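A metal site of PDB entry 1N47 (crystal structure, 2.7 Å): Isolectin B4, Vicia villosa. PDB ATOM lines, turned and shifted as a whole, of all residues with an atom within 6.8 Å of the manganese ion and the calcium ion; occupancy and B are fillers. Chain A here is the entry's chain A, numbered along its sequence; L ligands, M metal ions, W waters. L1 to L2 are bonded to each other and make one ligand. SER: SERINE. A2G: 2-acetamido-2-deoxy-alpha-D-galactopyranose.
Within 4 Å of the calcium ion: Asp 125, Tyr 127, Asn 129 and Asp 132.
Water W2 bridges O of Ile 145 (2.5 Å) and OE1 of Glu 123 (2.7 Å).
Four residues have an atom within 4 Å of the manganese ion: Glu 123, Asp 125, Asp 132 and His 137.
The backbone NH of Glu 123 sits at hydrogen-bond distance from the backbone carbonyl oxygen of Gly 139. OE1 of Glu 123 lies close to OD1 of Asp 141 (2.5 Å).
The calcium ion is bound by OD1 of Asp 132 (2.2 Å), OD1 of Asp 125 (2.4 Å), water W1 (2.5 Å), O of Tyr 127 (2.6 Å), OD2 of Asp 125 (2.6 Å) and OD1 of Asn 129 (2.7 Å).
The manganese ion is bound by the side-chain carboxylate of Asp 125, water W3, the side-chain carboxylate of Glu 123, the side-chain carboxylate of Asp 132, water W2 and a ring nitrogen (NE2) of His 137. The manganese ion has six donor atoms within binding distance.
OD1 of Asp 85 lies within hydrogen-bond range of O3 of A2G L2 (2.7 Å). N of SER L1 lies within hydrogen-bond range of OH of Tyr 127 (3.2 Å). The backbone NH (N) of Gly 103 lies within hydrogen-bond range of an oxygen (O3) of A2G L2, 3.2 Å away. The side-chain amide nitrogen of Asn 129 sits at hydrogen-bond distance from an oxygen (O3) of A2G L2 (2.9 Å).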
ATOM      1  N   ASP A  85     -19.076 -17.985   6.577  1.00  0.00           N
ATOM      2  CA  ASP A  85     -20.495 -18.359   6.527  1.00  0.00           C
ATOM      3  C   ASP A  85     -21.449 -17.197   6.839  1.00  0.00           C
ATOM      4  O   ASP A  85     -22.658 -17.395   6.753  1.00  0.00           O
ATOM      5  CB  ASP A  85     -20.826 -19.438   7.572  1.00  0.00           C
ATOM      6  CG  ASP A  85     -20.599 -20.852   7.066  1.00  0.00           C
ATOM      7  OD1 ASP A  85     -21.539 -21.458   6.479  1.00  0.00           O
ATOM      8  OD2 ASP A  85     -19.515 -21.448   7.256  1.00  0.00           O
ATOM      9  N   GLY A 103     -22.207 -23.264   9.463  1.00  0.00           N
ATOM     10  CA  GLY A 103     -23.452 -22.603   9.141  1.00  0.00           C
ATOM     11  C   GLY A 103     -24.372 -22.243  10.295  1.00  0.00           C
ATOM     12  O   GLY A 103     -25.479 -21.723  10.073  1.00  0.00           O
ATOM     13  N   PHE A 104     -23.950 -22.528  11.518  1.00  0.00           N
ATOM     14  CA  PHE A 104     -24.752 -22.181  12.695  1.00  0.00           C
ATOM     15  C   PHE A 104     -24.289 -20.851  13.296  1.00  0.00           C
ATOM     16  O   PHE A 104     -24.839 -20.357  14.277  1.00  0.00           O
ATOM     17  CB  PHE A 104     -24.716 -23.293  13.732  1.00  0.00           C
ATOM     18  CG  PHE A 104     -25.167 -24.617  13.211  1.00  0.00           C
ATOM     19  CD1 PHE A 104     -26.530 -24.933  13.149  1.00  0.00           C
ATOM     20  CD2 PHE A 104     -24.245 -25.546  12.777  1.00  0.00           C
ATOM     21  CE1 PHE A 104     -26.950 -26.185  12.645  1.00  0.00           C
ATOM     22  CE2 PHE A 104     -24.656 -26.787  12.275  1.00  0.00           C
ATOM     23  CZ  PHE A 104     -25.999 -27.109  12.205  1.00  0.00           C
ATOM     24  N   LEU A 105     -23.260 -20.267  12.699  1.00  0.00           N
ATOM     25  CA  LEU A 105     -22.758 -18.970  13.132  1.00  0.00           C
ATOM     26  C   LEU A 105     -22.480 -18.877  14.642  1.00  0.00           C
ATOM     27  O   LEU A 105     -22.317 -17.778  15.155  1.00  0.00           O
ATOM     28  CB  LEU A 105     -23.741 -17.878  12.722  1.00  0.00           C
ATOM     29  CG  LEU A 105     -24.587 -18.174  11.493  1.00  0.00           C
ATOM     30  CD1 LEU A 105     -25.909 -17.470  11.595  1.00  0.00           C
ATOM     31  CD2 LEU A 105     -23.876 -17.826  10.208  1.00  0.00           C
ATOM     32  N   GLU A 123     -29.243 -12.091  10.904  1.00  0.00           N
ATOM     33  CA  GLU A 123     -28.049 -12.565  10.235  1.00  0.00           C
ATOM     34  C   GLU A 123     -27.901 -11.957   8.876  1.00  0.00           C
ATOM     35  O   GLU A 123     -28.864 -11.589   8.247  1.00  0.00           O
ATOM     36  CB  GLU A 123     -28.104 -14.093  10.035  1.00  0.00           C
ATOM     37  CG  GLU A 123     -29.491 -14.641   9.650  1.00  0.00           C
ATOM     38  CD  GLU A 123     -29.475 -16.097   9.139  1.00  0.00           C
ATOM     39  OE1 GLU A 123     -29.492 -17.045   9.953  1.00  0.00           O
ATOM     40  OE2 GLU A 123     -29.458 -16.308   7.901  1.00  0.00           O
ATOM     41  N   ASP A 125     -26.295 -13.658   5.933  1.00  0.00           N
ATOM     42  CA  ASP A 125     -25.894 -15.022   5.572  1.00  0.00           C
ATOM     43  C   ASP A 125     -25.220 -15.140   4.200  1.00  0.00           C
ATOM     44  O   ASP A 125     -25.836 -14.813   3.169  1.00  0.00           O
ATOM     45  CB  ASP A 125     -27.180 -15.855   5.610  1.00  0.00           C
ATOM     46  CG  ASP A 125     -26.935 -17.324   5.803  1.00  0.00           C
ATOM     47  OD1 ASP A 125     -25.809 -17.772   5.500  1.00  0.00           O
ATOM     48  OD2 ASP A 125     -27.815 -18.109   6.236  1.00  0.00           O
ATOM     49  N   THR A 126     -23.965 -15.608   4.147  1.00  0.00           N
ATOM     50  CA  THR A 126     -23.241 -15.653   2.871  1.00  0.00           C
ATOM     51  C   THR A 126     -23.054 -17.021   2.205  1.00  0.00           C
ATOM     52  O   THR A 126     -22.330 -17.124   1.206  1.00  0.00           O
ATOM     53  CB  THR A 126     -21.864 -14.997   3.005  1.00  0.00           C
ATOM     54  OG1 THR A 126     -21.132 -15.650   4.041  1.00  0.00           O
ATOM     55  CG2 THR A 126     -21.978 -13.549   3.483  1.00  0.00           C
ATOM     56  N   TYR A 127     -23.703 -18.072   2.725  1.00  0.00           N
ATOM     57  CA  TYR A 127     -23.539 -19.395   2.121  1.00  0.00           C
ATOM     58  C   TYR A 127     -24.784 -20.236   2.295  1.00  0.00           C
ATOM     59  O   TYR A 127     -25.271 -20.425   3.405  1.00  0.00           O
ATOM     60  CB  TYR A 127     -22.323 -20.118   2.712  1.00  0.00           C
ATOM     61  CG  TYR A 127     -22.177 -21.559   2.264  1.00  0.00           C
ATOM     62  CD1 TYR A 127     -22.975 -22.560   2.808  1.00  0.00           C
ATOM     63  CD2 TYR A 127     -21.252 -21.912   1.282  1.00  0.00           C
ATOM     64  CE1 TYR A 127     -22.848 -23.866   2.404  1.00  0.00           C
ATOM     65  CE2 TYR A 127     -21.125 -23.216   0.865  1.00  0.00           C
ATOM     66  CZ  TYR A 127     -21.923 -24.203   1.439  1.00  0.00           C
ATOM     67  OH  TYR A 127     -21.809 -25.525   1.026  1.00  0.00           O
ATOM     68  N   SER A 128     -25.309 -20.765   1.187  1.00  0.00           N
ATOM     69  CA  SER A 128     -26.547 -21.490   1.276  1.00  0.00           C
ATOM     70  C   SER A 128     -26.374 -22.888   1.810  1.00  0.00           C
ATOM     71  O   SER A 128     -25.700 -23.712   1.176  1.00  0.00           O
ATOM     72  CB  SER A 128     -27.244 -21.549  -0.084  1.00  0.00           C
ATOM     73  OG  SER A 128     -27.380 -20.266  -0.646  1.00  0.00           O
ATOM     74  N   ASN A 129     -26.982 -23.124   2.962  1.00  0.00           N
ATOM     75  CA  ASN A 129     -27.070 -24.425   3.602  1.00  0.00           C
ATOM     76  C   ASN A 129     -28.406 -25.022   3.219  1.00  0.00           C
ATOM     77  O   ASN A 129     -29.162 -24.396   2.493  1.00  0.00           O
ATOM     78  CB  ASN A 129     -27.039 -24.294   5.130  1.00  0.00           C
ATOM     79  CG  ASN A 129     -25.682 -23.880   5.662  1.00  0.00           C
ATOM     80  OD1 ASN A 129     -25.472 -22.726   6.041  1.00  0.00           O
ATOM     81  ND2 ASN A 129     -24.750 -24.824   5.704  1.00  0.00           N
ATOM     82  N   TRP A 131     -31.078 -25.456   4.902  1.00  0.00           N
ATOM     83  CA  TRP A 131     -32.243 -24.754   5.472  1.00  0.00           C
ATOM     84  C   TRP A 131     -32.417 -23.337   4.875  1.00  0.00           C
ATOM     85  O   TRP A 131     -33.396 -22.633   5.179  1.00  0.00           O
ATOM     86  CB  TRP A 131     -32.122 -24.686   7.002  1.00  0.00           C
ATOM     87  CG  TRP A 131     -30.779 -24.183   7.437  1.00  0.00           C
ATOM     88  CD1 TRP A 131     -30.325 -22.887   7.399  1.00  0.00           C
ATOM     89  CD2 TRP A 131     -29.677 -24.963   7.918  1.00  0.00           C
ATOM     90  NE1 TRP A 131     -29.031 -22.824   7.827  1.00  0.00           N
ATOM     91  CE2 TRP A 131     -28.607 -24.092   8.164  1.00  0.00           C
ATOM     92  CE3 TRP A 131     -29.485 -26.342   8.164  1.00  0.00           C
ATOM     93  CZ2 TRP A 131     -27.375 -24.523   8.650  1.00  0.00           C
ATOM     94  CZ3 TRP A 131     -28.273 -26.765   8.643  1.00  0.00           C
ATOM     95  CH2 TRP A 131     -27.235 -25.870   8.891  1.00  0.00           C
ATOM     96  N   ASP A 132     -31.494 -22.948   4.016  1.00  0.00           N
ATOM     97  CA  ASP A 132     -31.480 -21.616   3.435  1.00  0.00           C
ATOM     98  C   ASP A 132     -32.042 -21.528   2.019  1.00  0.00           C
ATOM     99  O   ASP A 132     -32.255 -22.546   1.343  1.00  0.00           O
ATOM    100  CB  ASP A 132     -30.033 -21.116   3.395  1.00  0.00           C
ATOM    101  CG  ASP A 132     -29.543 -20.603   4.735  1.00  0.00           C
ATOM    102  OD1 ASP A 132     -28.308 -20.428   4.897  1.00  0.00           O
ATOM    103  OD2 ASP A 132     -30.328 -20.345   5.687  1.00  0.00           O
ATOM    104  N   PRO A 133     -32.310 -20.298   1.596  1.00  0.00           N
ATOM    105  CA  PRO A 133     -32.659 -20.000   0.198  1.00  0.00           C
ATOM    106  C   PRO A 133     -31.381 -20.059  -0.609  1.00  0.00           C
ATOM    107  O   PRO A 133     -30.302 -20.042  -0.014  1.00  0.00           O
ATOM    108  CB  PRO A 133     -33.132 -18.553   0.253  1.00  0.00           C
ATOM    109  CG  PRO A 133     -33.388 -18.308   1.674  1.00  0.00           C
ATOM    110  CD  PRO A 133     -32.333 -19.091   2.424  1.00  0.00           C
ATOM    111  N   HIS A 137     -28.443 -13.575   1.806  1.00  0.00           N
ATOM    112  CA  HIS A 137     -29.650 -12.992   2.367  1.00  0.00           C
ATOM    113  C   HIS A 137     -29.523 -12.515   3.792  1.00  0.00           C
ATOM    114  O   HIS A 137     -28.639 -12.929   4.541  1.00  0.00           O
ATOM    115  CB  HIS A 137     -30.722 -14.055   2.389  1.00  0.00           C
ATOM    116  CG  HIS A 137     -30.329 -15.255   3.176  1.00  0.00           C
ATOM    117  ND1 HIS A 137     -29.460 -16.199   2.689  1.00  0.00           N
ATOM    118  CD2 HIS A 137     -30.653 -15.657   4.428  1.00  0.00           C
ATOM    119  CE1 HIS A 137     -29.283 -17.149   3.594  1.00  0.00           C
ATOM    120  NE2 HIS A 137     -29.998 -16.845   4.660  1.00  0.00           N
ATOM    121  N   ILE A 138     -30.476 -11.670   4.165  1.00  0.00           N
ATOM    122  CA  ILE A 138     -30.623 -11.196   5.532  1.00  0.00           C
ATOM    123  C   ILE A 138     -31.784 -11.994   6.070  1.00  0.00           C
ATOM    124  O   ILE A 138     -32.778 -12.170   5.372  1.00  0.00           O
ATOM    125  CB  ILE A 138     -30.979  -9.726   5.550  1.00  0.00           C
ATOM    126  CG1 ILE A 138     -29.750  -8.874   5.199  1.00  0.00           C
ATOM    127  CG2 ILE A 138     -31.587  -9.357   6.892  1.00  0.00           C
ATOM    128  CD1 ILE A 138     -30.064  -7.365   5.031  1.00  0.00           C
ATOM    129  N   GLY A 139     -31.646 -12.514   7.277  1.00  0.00           N
ATOM    130  CA  GLY A 139     -32.710 -13.322   7.860  1.00  0.00           C
ATOM    131  C   GLY A 139     -32.910 -12.991   9.314  1.00  0.00           C
ATOM    132  O   GLY A 139     -32.002 -12.500  10.000  1.00  0.00           O
ATOM    133  N   ASP A 141     -33.637 -14.633  12.731  1.00  0.00           N
ATOM    134  CA  ASP A 141     -33.670 -15.874  13.472  1.00  0.00           C
ATOM    135  C   ASP A 141     -34.317 -15.721  14.836  1.00  0.00           C
ATOM    136  O   ASP A 141     -33.856 -14.934  15.632  1.00  0.00           O
ATOM    137  CB  ASP A 141     -32.233 -16.354  13.637  1.00  0.00           C
ATOM    138  CG  ASP A 141     -31.588 -16.728  12.317  1.00  0.00           C
ATOM    139  OD1 ASP A 141     -30.348 -16.821  12.254  1.00  0.00           O
ATOM    140  OD2 ASP A 141     -32.221 -16.929  11.276  1.00  0.00           O
ATOM    141  N   ILE A 145     -31.802 -21.615  13.493  1.00  0.00           N
ATOM    142  CA  ILE A 145     -31.024 -21.175  12.322  1.00  0.00           C
ATOM    143  C   ILE A 145     -31.898 -21.029  11.062  1.00  0.00           C
ATOM    144  O   ILE A 145     -31.485 -20.438  10.071  1.00  0.00           O
ATOM    145  CB  ILE A 145     -29.878 -22.192  12.090  1.00  0.00           C
ATOM    146  CG1 ILE A 145     -28.847 -21.670  11.107  1.00  0.00           C
ATOM    147  CG2 ILE A 145     -30.417 -23.537  11.628  1.00  0.00           C
ATOM    148  CD1 ILE A 145     -28.100 -20.489  11.633  1.00  0.00           C
ATOM    149  N   GLU A 146     -33.111 -21.586  11.101  1.00  0.00           N
ATOM    150  CA  GLU A 146     -34.049 -21.536   9.984  1.00  0.00           C
ATOM    151  C   GLU A 146     -34.866 -20.300  10.167  1.00  0.00           C
ATOM    152  O   GLU A 146     -35.892 -20.332  10.869  1.00  0.00           O
ATOM    153  CB  GLU A 146     -34.998 -22.736  10.035  1.00  0.00           C
ATOM    154  CG  GLU A 146     -35.511 -23.213   8.699  1.00  0.00           C
ATOM    155  CD  GLU A 146     -36.262 -24.554   8.781  1.00  0.00           C
ATOM    156  OE1 GLU A 146     -35.762 -25.523   9.449  1.00  0.00           O
ATOM    157  OE2 GLU A 146     -37.362 -24.661   8.174  1.00  0.00           O
ATOM    158  N   SER A 147     -34.441 -19.217   9.516  1.00  0.00           N
ATOM    159  CA  SER A 147     -35.053 -17.896   9.694  1.00  0.00           C
ATOM    160  C   SER A 147     -36.554 -17.876   9.556  1.00  0.00           C
ATOM    161  O   SER A 147     -37.122 -18.590   8.773  1.00  0.00           O
ATOM    162  CB  SER A 147     -34.442 -16.890   8.761  1.00  0.00           C
ATOM    163  OG  SER A 147     -33.052 -16.878   8.964  1.00  0.00           O
ATOM    164  N   THR A 150     -36.765 -13.939   5.553  1.00  0.00           N
ATOM    165  CA  THR A 150     -35.549 -13.501   4.893  1.00  0.00           C
ATOM    166  C   THR A 150     -35.878 -12.606   3.692  1.00  0.00           C
ATOM    167  O   THR A 150     -37.024 -12.589   3.228  1.00  0.00           O
ATOM    168  CB  THR A 150     -34.759 -14.690   4.352  1.00  0.00           C
ATOM    169  OG1 THR A 150     -35.485 -15.303   3.285  1.00  0.00           O
ATOM    170  CG2 THR A 150     -34.642 -15.810   5.376  1.00  0.00           C
HETATM  171  N   SER L   1     -22.829 -28.536   1.603  1.00  0.00           N
HETATM  172  CA  SER L   1     -22.503 -29.194   2.870  1.00  0.00           C
HETATM  173  C   SER L   1     -23.603 -28.977   3.922  1.00  0.00           C
HETATM  174  O   SER L   1     -24.395 -28.042   3.811  1.00  0.00           O
HETATM  175  CB  SER L   1     -21.138 -28.702   3.376  1.00  0.00           C
HETATM  176  OG  SER L   1     -21.250 -27.468   4.070  1.00  0.00           O
HETATM  177  OXT SER L   1     -23.716 -29.734   4.879  1.00  0.00           O
HETATM  178  O5  A2G L   2     -19.167 -26.613   4.683  1.00  0.00           O
HETATM  179  C1  A2G L   2     -20.366 -27.209   5.160  1.00  0.00           C
HETATM  180  C2  A2G L   2     -21.080 -26.290   6.155  1.00  0.00           C
HETATM  181  N2  A2G L   2     -22.251 -26.993   6.590  1.00  0.00           N
HETATM  182  C3  A2G L   2     -21.430 -24.993   5.467  1.00  0.00           C
HETATM  183  O3  A2G L   2     -22.031 -24.139   6.428  1.00  0.00           O
HETATM  184  C4  A2G L   2     -20.139 -24.363   5.011  1.00  0.00           C
HETATM  185  O4  A2G L   2     -19.359 -24.097   6.178  1.00  0.00           O
HETATM  186  C5  A2G L   2     -19.355 -25.315   4.114  1.00  0.00           C
HETATM  187  C6  A2G L   2     -17.981 -24.725   3.855  1.00  0.00           C
HETATM  188  O6  A2G L   2     -17.474 -25.268   2.632  1.00  0.00           O
HETATM  189  C7  A2G L   2     -22.532 -27.079   7.876  1.00  0.00           C
HETATM  190  O7  A2G L   2     -21.817 -26.540   8.698  1.00  0.00           O
HETATM  191  C8  A2G L   2     -23.758 -27.865   8.250  1.00  0.00           C
HETATM  192 MN    MN M   1     -29.691 -18.268   6.671  1.00  0.00          MN
HETATM  193 CA    CA M   2     -26.249 -20.150   5.752  1.00  0.00          CA
HETATM  194  O   HOH W   1     -23.890 -19.610   6.369  1.00  0.00           O
HETATM  195  O   HOH W   2     -29.556 -19.463   8.792  1.00  0.00           O
HETATM  196  O   HOH W   3     -31.772 -17.970   6.930  1.00  0.00           O
